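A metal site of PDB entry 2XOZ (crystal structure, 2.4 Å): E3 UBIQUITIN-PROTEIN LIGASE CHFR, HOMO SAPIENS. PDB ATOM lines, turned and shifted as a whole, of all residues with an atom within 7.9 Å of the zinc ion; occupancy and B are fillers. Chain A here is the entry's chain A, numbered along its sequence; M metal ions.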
ATOM      1  N   ASN A 150      12.129   3.617  23.608  1.00  0.00           N
ATOM      2  CA  ASN A 150      11.902   3.796  25.020  1.00  0.00           C
ATOM      3  C   ASN A 150      10.419   4.135  25.230  1.00  0.00           C
ATOM      4  O   ASN A 150       9.962   5.228  24.915  1.00  0.00           O
ATOM      5  CB  ASN A 150      12.855   4.862  25.556  1.00  0.00           C
ATOM      6  CG  ASN A 150      12.621   5.189  27.016  1.00  0.00           C
ATOM      7  OD1 ASN A 150      11.530   4.972  27.558  1.00  0.00           O
ATOM      8  ND2 ASN A 150      13.649   5.743  27.667  1.00  0.00           N
ATOM      9  N   PRO A 230      15.990  13.647  36.769  1.00  0.00           N
ATOM     10  CA  PRO A 230      17.374  13.978  36.425  1.00  0.00           C
ATOM     11  C   PRO A 230      17.763  13.395  35.071  1.00  0.00           C
ATOM     12  O   PRO A 230      17.315  12.294  34.733  1.00  0.00           O
ATOM     13  CB  PRO A 230      18.203  13.247  37.498  1.00  0.00           C
ATOM     14  CG  PRO A 230      17.238  12.768  38.531  1.00  0.00           C
ATOM     15  CD  PRO A 230      15.879  12.699  37.896  1.00  0.00           C
ATOM     16  N   ASP A 231      18.572  14.119  34.311  1.00  0.00           N
ATOM     17  CA  ASP A 231      19.167  13.592  33.087  1.00  0.00           C
ATOM     18  C   ASP A 231      19.999  12.336  33.352  1.00  0.00           C
ATOM     19  O   ASP A 231      20.800  12.301  34.287  1.00  0.00           O
ATOM     20  CB  ASP A 231      20.092  14.650  32.465  1.00  0.00           C
ATOM     21  CG  ASP A 231      19.325  15.782  31.792  1.00  0.00           C
ATOM     22  OD1 ASP A 231      18.088  15.675  31.617  1.00  0.00           O
ATOM     23  OD2 ASP A 231      19.966  16.788  31.421  1.00  0.00           O
ATOM     24  N   CYS A 232      19.835  11.314  32.534  1.00  0.00           N
ATOM     25  CA  CYS A 232      20.790  10.195  32.565  1.00  0.00           C
ATOM     26  C   CYS A 232      22.142  10.671  32.055  1.00  0.00           C
ATOM     27  O   CYS A 232      22.218  11.365  31.037  1.00  0.00           O
ATOM     28  CB  CYS A 232      20.334   8.991  31.737  1.00  0.00           C
ATOM     29  SG  CYS A 232      21.477   7.563  31.784  1.00  0.00           S
ATOM     30  N   TYR A 233      23.184  10.290  32.778  1.00  0.00           N
ATOM     31  CA  TYR A 233      24.559  10.577  32.388  1.00  0.00           C
ATOM     32  C   TYR A 233      24.809  10.134  30.941  1.00  0.00           C
ATOM     33  O   TYR A 233      25.507  10.817  30.187  1.00  0.00           O
ATOM     34  CB  TYR A 233      25.520   9.879  33.374  1.00  0.00           C
ATOM     35  CG  TYR A 233      26.989  10.209  33.154  1.00  0.00           C
ATOM     36  CD1 TYR A 233      27.772   9.426  32.299  1.00  0.00           C
ATOM     37  CD2 TYR A 233      27.592  11.268  33.797  1.00  0.00           C
ATOM     38  CE1 TYR A 233      29.104   9.725  32.081  1.00  0.00           C
ATOM     39  CE2 TYR A 233      28.947  11.562  33.588  1.00  0.00           C
ATOM     40  CZ  TYR A 233      29.689  10.793  32.732  1.00  0.00           C
ATOM     41  OH  TYR A 233      31.015  11.093  32.527  1.00  0.00           O
ATOM     42  N   TRP A 234      24.230   9.008  30.546  1.00  0.00           N
ATOM     43  CA  TRP A 234      24.523   8.426  29.231  1.00  0.00           C
ATOM     44  C   TRP A 234      23.637   8.951  28.103  1.00  0.00           C
ATOM     45  O   TRP A 234      23.862   8.633  26.950  1.00  0.00           O
ATOM     46  CB  TRP A 234      24.502   6.891  29.291  1.00  0.00           C
ATOM     47  CG  TRP A 234      25.266   6.349  30.457  1.00  0.00           C
ATOM     48  CD1 TRP A 234      24.753   5.929  31.645  1.00  0.00           C
ATOM     49  CD2 TRP A 234      26.699   6.234  30.577  1.00  0.00           C
ATOM     50  NE1 TRP A 234      25.768   5.541  32.487  1.00  0.00           N
ATOM     51  CE2 TRP A 234      26.973   5.706  31.856  1.00  0.00           C
ATOM     52  CE3 TRP A 234      27.764   6.501  29.711  1.00  0.00           C
ATOM     53  CZ2 TRP A 234      28.261   5.457  32.302  1.00  0.00           C
ATOM     54  CZ3 TRP A 234      29.052   6.252  30.157  1.00  0.00           C
ATOM     55  CH2 TRP A 234      29.285   5.733  31.442  1.00  0.00           C
ATOM     56  N   GLY A 235      22.636   9.774  28.438  1.00  0.00           N
ATOM     57  CA  GLY A 235      21.838  10.462  27.432  1.00  0.00           C
ATOM     58  C   GLY A 235      21.040   9.547  26.521  1.00  0.00           C
ATOM     59  O   GLY A 235      20.747   8.423  26.890  1.00  0.00           O
ATOM     60  N   ARG A 236      20.738  10.026  25.318  1.00  0.00           N
ATOM     61  CA  ARG A 236      19.776   9.373  24.418  1.00  0.00           C
ATOM     62  C   ARG A 236      20.157   7.959  24.004  1.00  0.00           C
ATOM     63  O   ARG A 236      19.283   7.139  23.703  1.00  0.00           O
ATOM     64  CB  ARG A 236      19.507  10.229  23.173  1.00  0.00           C
ATOM     65  CG  ARG A 236      20.756  10.495  22.318  1.00  0.00           C
ATOM     66  CD  ARG A 236      20.548  11.612  21.269  1.00  0.00           C
ATOM     67  NE  ARG A 236      19.605  11.259  20.206  1.00  0.00           N
ATOM     68  CZ  ARG A 236      19.419  11.990  19.092  1.00  0.00           C
ATOM     69  NH1 ARG A 236      20.127  13.092  18.893  1.00  0.00           N
ATOM     70  NH2 ARG A 236      18.535  11.604  18.168  1.00  0.00           N
ATOM     71  N   ASN A 237      21.459   7.672  23.971  1.00  0.00           N
ATOM     72  CA  ASN A 237      21.947   6.359  23.545  1.00  0.00           C
ATOM     73  C   ASN A 237      22.188   5.375  24.681  1.00  0.00           C
ATOM     74  O   ASN A 237      22.814   4.356  24.487  1.00  0.00           O
ATOM     75  CB  ASN A 237      23.218   6.485  22.684  1.00  0.00           C
ATOM     76  CG  ASN A 237      22.950   7.212  21.380  1.00  0.00           C
ATOM     77  OD1 ASN A 237      21.990   6.892  20.680  1.00  0.00           O
ATOM     78  ND2 ASN A 237      23.763   8.224  21.074  1.00  0.00           N
ATOM     79  N   CYS A 238      21.675   5.692  25.860  1.00  0.00           N
ATOM     80  CA  CYS A 238      21.815   4.811  27.011  1.00  0.00           C
ATOM     81  C   CYS A 238      21.266   3.424  26.720  1.00  0.00           C
ATOM     82  O   CYS A 238      20.162   3.284  26.181  1.00  0.00           O
ATOM     83  CB  CYS A 238      21.086   5.425  28.201  1.00  0.00           C
ATOM     84  SG  CYS A 238      21.124   4.395  29.641  1.00  0.00           S
ATOM     85  N   ARG A 239      22.013   2.402  27.075  1.00  0.00           N
ATOM     86  CA  ARG A 239      21.558   1.030  26.858  1.00  0.00           C
ATOM     87  C   ARG A 239      20.624   0.508  27.958  1.00  0.00           C
ATOM     88  O   ARG A 239      19.966  -0.493  27.783  1.00  0.00           O
ATOM     89  CB  ARG A 239      22.760   0.093  26.737  1.00  0.00           C
ATOM     90  CG  ARG A 239      23.824   0.580  25.773  1.00  0.00           C
ATOM     91  CD  ARG A 239      23.367   0.476  24.320  1.00  0.00           C
ATOM     92  NE  ARG A 239      24.115  -0.567  23.620  1.00  0.00           N
ATOM     93  CZ  ARG A 239      24.878  -0.341  22.548  1.00  0.00           C
ATOM     94  NH1 ARG A 239      25.545  -1.347  21.990  1.00  0.00           N
ATOM     95  NH2 ARG A 239      24.977   0.877  22.038  1.00  0.00           N
ATOM     96  N   THR A 240      20.571   1.187  29.094  1.00  0.00           N
ATOM     97  CA  THR A 240      19.780   0.671  30.211  1.00  0.00           C
ATOM     98  C   THR A 240      18.325   1.114  30.137  1.00  0.00           C
ATOM     99  O   THR A 240      17.498   0.623  30.896  1.00  0.00           O
ATOM    100  CB  THR A 240      20.346   1.109  31.564  1.00  0.00           C
ATOM    101  OG1 THR A 240      21.769   1.039  31.519  1.00  0.00           O
ATOM    102  CG2 THR A 240      19.802   0.213  32.694  1.00  0.00           C
ATOM    103  N   GLN A 241      18.029   2.035  29.241  1.00  0.00           N
ATOM    104  CA  GLN A 241      16.693   2.636  29.210  1.00  0.00           C
ATOM    105  C   GLN A 241      15.586   1.690  28.653  1.00  0.00           C
ATOM    106  O   GLN A 241      14.413   2.040  28.633  1.00  0.00           O
ATOM    107  CB  GLN A 241      16.720   3.967  28.459  1.00  0.00           C
ATOM    108  CG  GLN A 241      16.926   3.787  27.009  1.00  0.00           C
ATOM    109  CD  GLN A 241      17.053   5.091  26.276  1.00  0.00           C
ATOM    110  OE1 GLN A 241      16.156   5.938  26.315  1.00  0.00           O
ATOM    111  NE2 GLN A 241      18.170   5.270  25.580  1.00  0.00           N
ATOM    112  N   VAL A 242      15.959   0.489  28.237  1.00  0.00           N
ATOM    113  CA  VAL A 242      14.954  -0.492  27.865  1.00  0.00           C
ATOM    114  C   VAL A 242      14.418  -1.231  29.088  1.00  0.00           C
ATOM    115  O   VAL A 242      13.562  -2.111  28.980  1.00  0.00           O
ATOM    116  CB  VAL A 242      15.477  -1.520  26.827  1.00  0.00           C
ATOM    117  CG1 VAL A 242      15.884  -0.806  25.511  1.00  0.00           C
ATOM    118  CG2 VAL A 242      16.620  -2.343  27.405  1.00  0.00           C
ATOM    119  N   HIS A 246      14.681   2.152  35.185  1.00  0.00           N
ATOM    120  CA  HIS A 246      15.661   3.138  34.772  1.00  0.00           C
ATOM    121  C   HIS A 246      14.998   4.198  33.870  1.00  0.00           C
ATOM    122  O   HIS A 246      15.232   5.391  34.028  1.00  0.00           O
ATOM    123  CB  HIS A 246      16.824   2.447  34.035  1.00  0.00           C
ATOM    124  CG  HIS A 246      17.927   3.384  33.634  1.00  0.00           C
ATOM    125  ND1 HIS A 246      18.892   3.801  34.520  1.00  0.00           N
ATOM    126  CD2 HIS A 246      18.195   3.988  32.461  1.00  0.00           C
ATOM    127  CE1 HIS A 246      19.714   4.632  33.904  1.00  0.00           C
ATOM    128  NE2 HIS A 246      19.320   4.753  32.657  1.00  0.00           N
ATOM    129  N   ALA A 247      14.177   3.735  32.937  1.00  0.00           N
ATOM    130  CA  ALA A 247      13.519   4.613  31.973  1.00  0.00           C
ATOM    131  C   ALA A 247      12.591   5.610  32.651  1.00  0.00           C
ATOM    132  O   ALA A 247      12.511   6.763  32.242  1.00  0.00           O
ATOM    133  CB  ALA A 247      12.766   3.803  30.891  1.00  0.00           C
ATOM    134  N   PHE A 250      15.003   8.274  35.084  1.00  0.00           N
ATOM    135  CA  PHE A 250      15.855   9.295  34.459  1.00  0.00           C
ATOM    136  C   PHE A 250      15.301   9.809  33.133  1.00  0.00           C
ATOM    137  O   PHE A 250      14.646   9.068  32.404  1.00  0.00           O
ATOM    138  CB  PHE A 250      17.253   8.780  34.167  1.00  0.00           C
ATOM    139  CG  PHE A 250      18.036   8.404  35.382  1.00  0.00           C
ATOM    140  CD1 PHE A 250      18.178   7.074  35.758  1.00  0.00           C
ATOM    141  CD2 PHE A 250      18.676   9.377  36.137  1.00  0.00           C
ATOM    142  CE1 PHE A 250      18.925   6.712  36.860  1.00  0.00           C
ATOM    143  CE2 PHE A 250      19.427   9.020  37.255  1.00  0.00           C
ATOM    144  CZ  PHE A 250      19.542   7.684  37.613  1.00  0.00           C
ATOM    145  N   ASN A 251      15.600  11.066  32.827  1.00  0.00           N
ATOM    146  CA  ASN A 251      15.280  11.633  31.527  1.00  0.00           C
ATOM    147  C   ASN A 251      16.335  11.215  30.496  1.00  0.00           C
ATOM    148  O   ASN A 251      17.530  11.288  30.771  1.00  0.00           O
ATOM    149  CB  ASN A 251      15.187  13.158  31.636  1.00  0.00           C
ATOM    150  CG  ASN A 251      15.211  13.850  30.280  1.00  0.00           C
ATOM    151  OD1 ASN A 251      14.488  13.474  29.349  1.00  0.00           O
ATOM    152  ND2 ASN A 251      16.078  14.854  30.156  1.00  0.00           N
ATOM    153  N   HIS A 252      15.897  10.749  29.347  1.00  0.00           N
ATOM    154  CA  HIS A 252      16.815  10.331  28.278  1.00  0.00           C
ATOM    155  C   HIS A 252      16.656  11.171  27.008  1.00  0.00           C
ATOM    156  O   HIS A 252      17.162  10.794  25.960  1.00  0.00           O
ATOM    157  CB  HIS A 252      16.636   8.852  27.954  1.00  0.00           C
ATOM    158  CG  HIS A 252      17.207   7.943  29.008  1.00  0.00           C
ATOM    159  ND1 HIS A 252      16.443   7.471  30.057  1.00  0.00           N
ATOM    160  CD2 HIS A 252      18.446   7.442  29.177  1.00  0.00           C
ATOM    161  CE1 HIS A 252      17.206   6.716  30.825  1.00  0.00           C
ATOM    162  NE2 HIS A 252      18.418   6.672  30.325  1.00  0.00           N
ATOM    163  N   CYS A 254      18.274  13.824  26.157  1.00  0.00           N
ATOM    164  CA  CYS A 254      19.450  14.654  26.414  1.00  0.00           C
ATOM    165  C   CYS A 254      20.641  13.939  25.797  1.00  0.00           C
ATOM    166  O   CYS A 254      20.517  12.797  25.389  1.00  0.00           O
ATOM    167  CB  CYS A 254      19.669  14.883  27.912  1.00  0.00           C
ATOM    168  SG  CYS A 254      19.871  13.367  28.923  1.00  0.00           S
HETATM  169 ZN    ZN M   1      20.014   5.871  31.168  1.00  0.00          ZN
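Within 4 Å of the zinc ion: Cys 232, Cys 238, His 246 and His 252. The nearest printed residue that does not touch the zinc ion is Gln 241 (4.7 Å).
The backbone carbonyl oxygen (O) of Phe 250 sits at hydrogen-bond distance from a ring nitrogen (ND1) of His 252 (3.4 Å). SG of Cys 232 sits close to N of Trp 234, at 3.3 Å. N of Cys 232 is in hydrogen-bond range of O of Asn 251. The backbone carbonyl oxygen (O) of Cys 232 lies within hydrogen-bond range of the side-chain sulfur (SG) of Cys 254, 3.7 Å away. The side-chain amide nitrogen of Gln 241 is in hydrogen-bond range of the backbone carbonyl oxygen of Cys 238. SG of Cys 238 lies close to N of Thr 240 (3.3 Å).
The zinc ion is bound by a ring nitrogen (NE2) of His 252 (2.0 Å), a ring nitrogen (NE2) of His 246 (2.0 Å), the side-chain sulfur (SG) of Cys 232 (2.3 Å) and the side-chain sulfur (SG) of Cys 238 (2.4 Å).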
